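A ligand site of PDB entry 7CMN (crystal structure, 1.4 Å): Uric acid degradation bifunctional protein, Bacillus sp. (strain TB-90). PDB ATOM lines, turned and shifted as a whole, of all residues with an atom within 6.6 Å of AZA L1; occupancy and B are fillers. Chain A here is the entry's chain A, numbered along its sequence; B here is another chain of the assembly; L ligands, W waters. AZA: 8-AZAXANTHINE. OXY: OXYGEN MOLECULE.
Water W1 bridges a nitrogen (N9) of AZA L1 and the guanidinium group of Arg 195.
N of Ile 243 lies within hydrogen-bond range of O2 of AZA L1. The side-chain amide oxygen (OE1) of Gln 244 is in hydrogen-bond range of a nitrogen (N1) of AZA L1, at 2.9 Å. N of Thr 67 of chain B lies within hydrogen-bond range of N7 of AZA L1 (2.9 Å). N7 of AZA L1 lies within hydrogen-bond range of OG1 of Thr 67 of chain B, 3.2 Å away. The side-chain amide nitrogen (ND2) of Asn 270 lies within hydrogen-bond range of an oxygen (O2) of OXY L2. The side-chain hydroxyl (OG1) of Thr 67 of chain B lies within hydrogen-bond range of an oxygen (O2) of OXY L2, 2.8 Å away. A nitrogen (N3) of AZA L1 lies close to the side-chain amide nitrogen of Asn 270, 3.4 Å away. NE2 of Gln 298 sits at hydrogen-bond distance from O1 of OXY L2 (2.8 Å). NH2 of Arg 195 sits at hydrogen-bond distance from O2 of AZA L1, at 2.8 Å.
An oxygen (O2) of OXY L2 sits close to a nitrogen (N3) of AZA L1 (3.4 Å).
The side-chain hydroxyl of Thr 67 of chain B is in hydrogen-bond range of the side-chain amino group of Lys 7 of chain B (3.4 Å). N of Gln 244 sits close to OG of Ser 242 (3.5 Å). OH of Tyr 5 of chain B lies within hydrogen-bond range of O of Val 65 of chain B, 2.7 Å away. N of Asn 270 sits at hydrogen-bond distance from O of Gly 296, at 2.8 Å.
Phe 178 touches AZA L1. Leu 189 touches AZA L1 (CD2 to N8, 3.7 Å). Ser 242 touches AZA L1 (CA to O2, 3.4 Å). NE2 of Gln 298 touches N1 of AZA L1 (3.9 Å). Tyr 5 of chain B touches AZA L1. Val 64 of chain B touches AZA L1 (CG1 to O6, 3.9 Å). Ala 66 of chain B touches AZA L1 (CA to N7, 3.6 Å). N of Asp 68 of chain B touches N8 of AZA L1, 3.9 Å away. Hydrophobic or aromatic side chains within 4 Å of AZA L1: Phe 178, Leu 189, Ile 243, Tyr 5 of chain B, Val 64 of chain B and Ala 66 of chain B. 13 residues have an atom within 4 Å of AZA L1: Phe 178, Leu 189, Arg 195, Ser 242, Ile 243, Gln 244, Asn 270, Gln 298, Tyr 5 of chain B, Val 64 of chain B, Ala 66 of chain B, Thr 67 of chain B and Asp 68 of chain B. The nearest printed residue that does not touch AZA L1 is Val 65 of chain B (4.7 Å).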
ATOM      1  N   SER A 177       3.181  28.562  38.634  1.00  0.00           N
ATOM      2  CA  SER A 177       3.710  29.636  37.834  1.00  0.00           C
ATOM      3  C   SER A 177       3.444  29.347  36.345  1.00  0.00           C
ATOM      4  O   SER A 177       3.250  28.196  35.949  1.00  0.00           O
ATOM      5  CB  SER A 177       5.212  29.824  38.050  1.00  0.00           C
ATOM      6  OG  SER A 177       5.965  28.863  37.353  1.00  0.00           O
ATOM      7  N   PHE A 178       3.418  30.411  35.557  1.00  0.00           N
ATOM      8  CA  PHE A 178       3.423  30.291  34.084  1.00  0.00           C
ATOM      9  C   PHE A 178       4.247  31.468  33.568  1.00  0.00           C
ATOM     10  O   PHE A 178       3.738  32.591  33.467  1.00  0.00           O
ATOM     11  CB  PHE A 178       2.044  30.235  33.460  1.00  0.00           C
ATOM     12  CG  PHE A 178       2.078  29.872  31.998  1.00  0.00           C
ATOM     13  CD1 PHE A 178       2.638  28.667  31.585  1.00  0.00           C
ATOM     14  CD2 PHE A 178       1.595  30.738  31.057  1.00  0.00           C
ATOM     15  CE1 PHE A 178       2.700  28.348  30.236  1.00  0.00           C
ATOM     16  CE2 PHE A 178       1.644  30.425  29.705  1.00  0.00           C
ATOM     17  CZ  PHE A 178       2.208  29.217  29.301  1.00  0.00           C
ATOM     18  N   PHE A 181       7.198  31.889  28.504  1.00  0.00           N
ATOM     19  CA  PHE A 181       6.578  31.566  27.219  1.00  0.00           C
ATOM     20  C   PHE A 181       6.913  32.624  26.183  1.00  0.00           C
ATOM     21  O   PHE A 181       7.470  33.674  26.468  1.00  0.00           O
ATOM     22  CB  PHE A 181       5.073  31.349  27.384  1.00  0.00           C
ATOM     23  CG  PHE A 181       4.362  32.451  28.123  1.00  0.00           C
ATOM     24  CD1 PHE A 181       3.785  33.516  27.446  1.00  0.00           C
ATOM     25  CD2 PHE A 181       4.237  32.419  29.516  1.00  0.00           C
ATOM     26  CE1 PHE A 181       3.110  34.513  28.109  1.00  0.00           C
ATOM     27  CE2 PHE A 181       3.558  33.415  30.193  1.00  0.00           C
ATOM     28  CZ  PHE A 181       3.022  34.474  29.506  1.00  0.00           C
ATOM     29  N   LEU A 189      -0.511  38.222  27.413  1.00  0.00           N
ATOM     30  CA  LEU A 189      -0.642  37.588  28.715  1.00  0.00           C
ATOM     31  C   LEU A 189       0.567  37.906  29.583  1.00  0.00           C
ATOM     32  O   LEU A 189       1.704  37.676  29.162  1.00  0.00           O
ATOM     33  CB  LEU A 189      -0.760  36.062  28.536  1.00  0.00           C
ATOM     34  CG  LEU A 189      -0.881  35.261  29.855  1.00  0.00           C
ATOM     35  CD1 LEU A 189      -2.228  35.518  30.497  1.00  0.00           C
ATOM     36  CD2 LEU A 189      -0.680  33.770  29.610  1.00  0.00           C
ATOM     37  N   ARG A 195      -0.060  31.906  40.446  1.00  0.00           N
ATOM     38  CA  ARG A 195      -1.420  32.000  39.997  1.00  0.00           C
ATOM     39  C   ARG A 195      -2.266  30.901  40.629  1.00  0.00           C
ATOM     40  O   ARG A 195      -1.741  29.844  40.989  1.00  0.00           O
ATOM     41  CB  ARG A 195      -1.491  31.837  38.470  1.00  0.00           C
ATOM     42  CG  ARG A 195      -1.014  30.461  37.987  1.00  0.00           C
ATOM     43  CD  ARG A 195      -1.082  30.377  36.457  1.00  0.00           C
ATOM     44  NE  ARG A 195      -0.680  29.073  35.970  1.00  0.00           N
ATOM     45  CZ  ARG A 195      -0.821  28.679  34.698  1.00  0.00           C
ATOM     46  NH1 ARG A 195      -1.355  29.485  33.791  1.00  0.00           N
ATOM     47  NH2 ARG A 195      -0.437  27.458  34.351  1.00  0.00           N
ATOM     48  N   LEU A 197      -4.057  28.277  39.753  1.00  0.00           N
ATOM     49  CA  LEU A 197      -4.345  27.475  38.564  1.00  0.00           C
ATOM     50  C   LEU A 197      -5.590  26.634  38.774  1.00  0.00           C
ATOM     51  O   LEU A 197      -5.700  25.884  39.752  1.00  0.00           O
ATOM     52  CB  LEU A 197      -3.145  26.576  38.275  1.00  0.00           C
ATOM     53  CG  LEU A 197      -3.324  25.549  37.151  1.00  0.00           C
ATOM     54  CD1 LEU A 197      -3.600  26.217  35.834  1.00  0.00           C
ATOM     55  CD2 LEU A 197      -2.061  24.681  37.059  1.00  0.00           C
ATOM     56  N   LEU A 241       4.692  24.413  36.743  1.00  0.00           N
ATOM     57  CA  LEU A 241       5.238  25.392  35.810  1.00  0.00           C
ATOM     58  C   LEU A 241       4.328  25.605  34.600  1.00  0.00           C
ATOM     59  O   LEU A 241       4.619  26.502  33.802  1.00  0.00           O
ATOM     60  CB  LEU A 241       6.616  24.919  35.322  1.00  0.00           C
ATOM     61  CG  LEU A 241       7.682  24.773  36.427  1.00  0.00           C
ATOM     62  CD1 LEU A 241       8.867  24.002  35.866  1.00  0.00           C
ATOM     63  CD2 LEU A 241       8.096  26.136  36.928  1.00  0.00           C
ATOM     64  N   SER A 242       3.269  24.818  34.469  1.00  0.00           N
ATOM     65  CA  SER A 242       2.272  24.918  33.419  1.00  0.00           C
ATOM     66  C   SER A 242       1.326  23.731  33.655  1.00  0.00           C
ATOM     67  O   SER A 242       1.627  22.837  34.445  1.00  0.00           O
ATOM     68  CB  SER A 242       2.906  24.797  32.036  1.00  0.00           C
ATOM     69  OG  SER A 242       3.520  23.531  31.857  1.00  0.00           O
ATOM     70  N   ILE A 243       0.205  23.724  32.940  1.00  0.00           N
ATOM     71  CA  ILE A 243      -0.636  22.520  33.000  1.00  0.00           C
ATOM     72  C   ILE A 243       0.082  21.352  32.348  1.00  0.00           C
ATOM     73  O   ILE A 243       0.027  20.218  32.835  1.00  0.00           O
ATOM     74  CB  ILE A 243      -1.997  22.793  32.331  1.00  0.00           C
ATOM     75  CG1 ILE A 243      -2.750  23.889  33.088  1.00  0.00           C
ATOM     76  CG2 ILE A 243      -2.841  21.519  32.291  1.00  0.00           C
ATOM     77  CD1 ILE A 243      -3.914  24.471  32.316  1.00  0.00           C
ATOM     78  N   GLN A 244       0.731  21.609  31.194  1.00  0.00           N
ATOM     79  CA  GLN A 244       1.573  20.607  30.543  1.00  0.00           C
ATOM     80  C   GLN A 244       2.499  19.929  31.542  1.00  0.00           C
ATOM     81  O   GLN A 244       2.600  18.693  31.576  1.00  0.00           O
ATOM     82  CB  GLN A 244       2.373  21.268  29.433  1.00  0.00           C
ATOM     83  CG  GLN A 244       1.534  21.771  28.243  1.00  0.00           C
ATOM     84  CD  GLN A 244       1.126  23.230  28.360  1.00  0.00           C
ATOM     85  OE1 GLN A 244       0.778  23.732  29.449  1.00  0.00           O
ATOM     86  NE2 GLN A 244       1.086  23.929  27.217  1.00  0.00           N
ATOM     87  N   ASN A 270      -7.737  24.854  30.889  1.00  0.00           N
ATOM     88  CA  ASN A 270      -7.361  25.956  31.772  1.00  0.00           C
ATOM     89  C   ASN A 270      -8.577  26.858  31.976  1.00  0.00           C
ATOM     90  O   ASN A 270      -9.141  27.376  30.994  1.00  0.00           O
ATOM     91  CB  ASN A 270      -6.226  26.761  31.159  1.00  0.00           C
ATOM     92  CG  ASN A 270      -5.632  27.752  32.116  1.00  0.00           C
ATOM     93  OD1 ASN A 270      -6.223  28.076  33.161  1.00  0.00           O
ATOM     94  ND2 ASN A 270      -4.455  28.255  31.780  1.00  0.00           N
ATOM     95  N   GLY A 296      -7.842  27.522  27.333  1.00  0.00           N
ATOM     96  CA  GLY A 296      -6.761  26.670  26.871  1.00  0.00           C
ATOM     97  C   GLY A 296      -7.016  25.206  27.178  1.00  0.00           C
ATOM     98  O   GLY A 296      -7.751  24.836  28.087  1.00  0.00           O
ATOM     99  N   PHE A 297      -6.379  24.333  26.385  1.00  0.00           N
ATOM    100  CA  PHE A 297      -6.470  22.908  26.654  1.00  0.00           C
ATOM    101  C   PHE A 297      -5.200  22.218  26.219  1.00  0.00           C
ATOM    102  O   PHE A 297      -4.431  22.736  25.395  1.00  0.00           O
ATOM    103  CB  PHE A 297      -7.696  22.269  25.965  1.00  0.00           C
ATOM    104  CG  PHE A 297      -7.672  22.370  24.471  1.00  0.00           C
ATOM    105  CD1 PHE A 297      -6.951  21.447  23.722  1.00  0.00           C
ATOM    106  CD2 PHE A 297      -8.344  23.377  23.814  1.00  0.00           C
ATOM    107  CE1 PHE A 297      -6.918  21.544  22.341  1.00  0.00           C
ATOM    108  CE2 PHE A 297      -8.320  23.468  22.424  1.00  0.00           C
ATOM    109  CZ  PHE A 297      -7.602  22.565  21.697  1.00  0.00           C
ATOM    110  N   GLN A 298      -4.966  21.045  26.812  1.00  0.00           N
ATOM    111  CA  GLN A 298      -3.801  20.219  26.523  1.00  0.00           C
ATOM    112  C   GLN A 298      -4.267  18.775  26.393  1.00  0.00           C
ATOM    113  O   GLN A 298      -5.276  18.375  26.991  1.00  0.00           O
ATOM    114  CB  GLN A 298      -2.764  20.321  27.654  1.00  0.00           C
ATOM    115  CG  GLN A 298      -2.212  21.717  27.865  1.00  0.00           C
ATOM    116  CD  GLN A 298      -3.183  22.648  28.571  1.00  0.00           C
ATOM    117  OE1 GLN A 298      -4.118  22.216  29.262  1.00  0.00           O
ATOM    118  NE2 GLN A 298      -2.968  23.957  28.406  1.00  0.00           N
ATOM    119  N   TYR B   5      -1.882  20.919  22.113  1.00  0.00           N
ATOM    120  CA  TYR B   5      -2.511  21.866  23.031  1.00  0.00           C
ATOM    121  C   TYR B   5      -3.059  23.003  22.204  1.00  0.00           C
ATOM    122  O   TYR B   5      -2.741  23.157  21.021  1.00  0.00           O
ATOM    123  CB  TYR B   5      -1.508  22.322  24.118  1.00  0.00           C
ATOM    124  CG  TYR B   5      -0.575  23.419  23.682  1.00  0.00           C
ATOM    125  CD1 TYR B   5       0.390  23.191  22.700  1.00  0.00           C
ATOM    126  CD2 TYR B   5      -0.614  24.681  24.273  1.00  0.00           C
ATOM    127  CE1 TYR B   5       1.267  24.181  22.316  1.00  0.00           C
ATOM    128  CE2 TYR B   5       0.243  25.673  23.875  1.00  0.00           C
ATOM    129  CZ  TYR B   5       1.179  25.420  22.862  1.00  0.00           C
ATOM    130  OH  TYR B   5       2.056  26.415  22.455  1.00  0.00           O
ATOM    131  N   GLY B   6      -3.911  23.810  22.835  1.00  0.00           N
ATOM    132  CA  GLY B   6      -4.517  24.910  22.055  1.00  0.00           C
ATOM    133  C   GLY B   6      -5.557  25.678  22.843  1.00  0.00           C
ATOM    134  O   GLY B   6      -5.482  25.799  24.052  1.00  0.00           O
ATOM    135  N   LYS B   7      -6.523  26.200  22.104  1.00  0.00           N
ATOM    136  CA  LYS B   7      -7.486  27.141  22.680  1.00  0.00           C
ATOM    137  C   LYS B   7      -8.848  26.824  22.077  1.00  0.00           C
ATOM    138  O   LYS B   7      -8.981  26.678  20.849  1.00  0.00           O
ATOM    139  CB  LYS B   7      -7.085  28.572  22.347  1.00  0.00           C
ATOM    140  CG  LYS B   7      -7.756  29.633  23.192  1.00  0.00           C
ATOM    141  CD  LYS B   7      -7.152  29.685  24.569  1.00  0.00           C
ATOM    142  CE  LYS B   7      -7.657  30.848  25.342  1.00  0.00           C
ATOM    143  NZ  LYS B   7      -6.934  30.906  26.629  1.00  0.00           N
ATOM    144  N   ASN B  61       8.980  26.380  28.978  1.00  0.00           N
ATOM    145  CA  ASN B  61       8.008  27.112  28.168  1.00  0.00           C
ATOM    146  C   ASN B  61       8.657  27.897  27.041  1.00  0.00           C
ATOM    147  O   ASN B  61       7.956  28.673  26.357  1.00  0.00           O
ATOM    148  CB  ASN B  61       7.199  28.046  29.083  1.00  0.00           C
ATOM    149  CG  ASN B  61       6.349  27.277  30.063  1.00  0.00           C
ATOM    150  OD1 ASN B  61       5.767  26.240  29.713  1.00  0.00           O
ATOM    151  ND2 ASN B  61       6.292  27.763  31.304  1.00  0.00           N
ATOM    152  N   VAL B  64       6.690  27.577  23.890  1.00  0.00           N
ATOM    153  CA  VAL B  64       5.240  27.528  24.102  1.00  0.00           C
ATOM    154  C   VAL B  64       4.656  28.841  23.619  1.00  0.00           C
ATOM    155  O   VAL B  64       4.905  29.896  24.197  1.00  0.00           O
ATOM    156  CB  VAL B  64       4.893  27.275  25.566  1.00  0.00           C
ATOM    157  CG1 VAL B  64       3.398  27.504  25.801  1.00  0.00           C
ATOM    158  CG2 VAL B  64       5.302  25.881  25.977  1.00  0.00           C
ATOM    159  N   VAL B  65       3.857  28.779  22.546  1.00  0.00           N
ATOM    160  CA  VAL B  65       2.944  29.853  22.213  1.00  0.00           C
ATOM    161  C   VAL B  65       1.807  29.805  23.241  1.00  0.00           C
ATOM    162  O   VAL B  65       1.103  28.792  23.365  1.00  0.00           O
ATOM    163  CB  VAL B  65       2.406  29.719  20.793  1.00  0.00           C
ATOM    164  CG1 VAL B  65       1.392  30.827  20.476  1.00  0.00           C
ATOM    165  CG2 VAL B  65       3.534  29.711  19.782  1.00  0.00           C
ATOM    166  N   ALA B  66       1.650  30.876  24.009  1.00  0.00           N
ATOM    167  CA  ALA B  66       0.576  30.875  24.991  1.00  0.00           C
ATOM    168  C   ALA B  66      -0.764  30.657  24.289  1.00  0.00           C
ATOM    169  O   ALA B  66      -1.039  31.178  23.194  1.00  0.00           O
ATOM    170  CB  ALA B  66       0.561  32.188  25.784  1.00  0.00           C
ATOM    171  N   THR B  67      -1.614  29.825  24.896  1.00  0.00           N
ATOM    172  CA  THR B  67      -2.952  29.639  24.315  1.00  0.00           C
ATOM    173  C   THR B  67      -3.704  30.962  24.264  1.00  0.00           C
ATOM    174  O   THR B  67      -4.476  31.191  23.316  1.00  0.00           O
ATOM    175  CB  THR B  67      -3.730  28.580  25.087  1.00  0.00           C
ATOM    176  OG1 THR B  67      -4.077  29.051  26.389  1.00  0.00           O
ATOM    177  CG2 THR B  67      -2.952  27.289  25.199  1.00  0.00           C
ATOM    178  N   ASP B  68      -3.436  31.850  25.237  1.00  0.00           N
ATOM    179  CA  ASP B  68      -4.020  33.188  25.206  1.00  0.00           C
ATOM    180  C   ASP B  68      -3.582  33.953  23.957  1.00  0.00           C
ATOM    181  O   ASP B  68      -4.367  34.716  23.380  1.00  0.00           O
ATOM    182  CB  ASP B  68      -3.619  33.951  26.478  1.00  0.00           C
ATOM    183  CG  ASP B  68      -4.242  35.319  26.563  1.00  0.00           C
ATOM    184  OD1 ASP B  68      -5.424  35.412  26.994  1.00  0.00           O
ATOM    185  OD2 ASP B  68      -3.589  36.315  26.194  1.00  0.00           O
ATOM    186  N   SER B  69      -2.337  33.762  23.525  1.00  0.00           N
ATOM    187  CA  SER B  69      -1.841  34.386  22.330  1.00  0.00           C
ATOM    188  C   SER B  69      -2.490  33.799  21.076  1.00  0.00           C
ATOM    189  O   SER B  69      -2.729  34.506  20.103  1.00  0.00           O
ATOM    190  CB  SER B  69      -0.327  34.233  22.238  1.00  0.00           C
ATOM    191  OG  SER B  69       0.292  34.804  23.417  1.00  0.00           O
ATOM    192  N   MET B  70      -2.779  32.502  21.079  1.00  0.00           N
ATOM    193  CA  MET B  70      -3.496  31.929  19.923  1.00  0.00           C
ATOM    194  C   MET B  70      -4.866  32.571  19.765  1.00  0.00           C
ATOM    195  O   MET B  70      -5.373  32.715  18.641  1.00  0.00           O
ATOM    196  CB  MET B  70      -3.651  30.423  20.081  1.00  0.00           C
ATOM    197  CG  MET B  70      -2.385  29.670  20.431  1.00  0.00           C
ATOM    198  SD  MET B  70      -2.759  27.947  20.684  1.00  0.00           S
ATOM    199  CE  MET B  70      -1.164  27.239  21.074  1.00  0.00           C
HETATM  200  N1  AZA L   1      -0.186  26.436  29.648  1.00  0.00           N
HETATM  201  C2  AZA L   1      -0.600  26.890  30.856  1.00  0.00           C
HETATM  202  O2  AZA L   1      -0.441  26.235  31.829  1.00  0.00           O
HETATM  203  N3  AZA L   1      -1.154  28.107  30.961  1.00  0.00           N
HETATM  204  C4  AZA L   1      -1.323  28.870  29.872  1.00  0.00           C
HETATM  205  C5  AZA L   1      -0.909  28.428  28.658  1.00  0.00           C
HETATM  206  C6  AZA L   1      -0.364  27.186  28.534  1.00  0.00           C
HETATM  207  O6  AZA L   1       0.008  26.798  27.495  1.00  0.00           O
HETATM  208  N7  AZA L   1      -1.193  29.392  27.760  1.00  0.00           N
HETATM  209  N8  AZA L   1      -1.780  30.425  28.421  1.00  0.00           N
HETATM  210  N9  AZA L   1      -1.825  30.096  29.742  1.00  0.00           N
HETATM  211  O1  OXY L   2      -4.004  26.529  28.939  1.00  0.00           O
HETATM  212  O2  OXY L   2      -3.715  27.630  28.719  1.00  0.00           O
HETATM  213  O   HOH W   1      -2.969  31.550  31.796  1.00  0.00           O
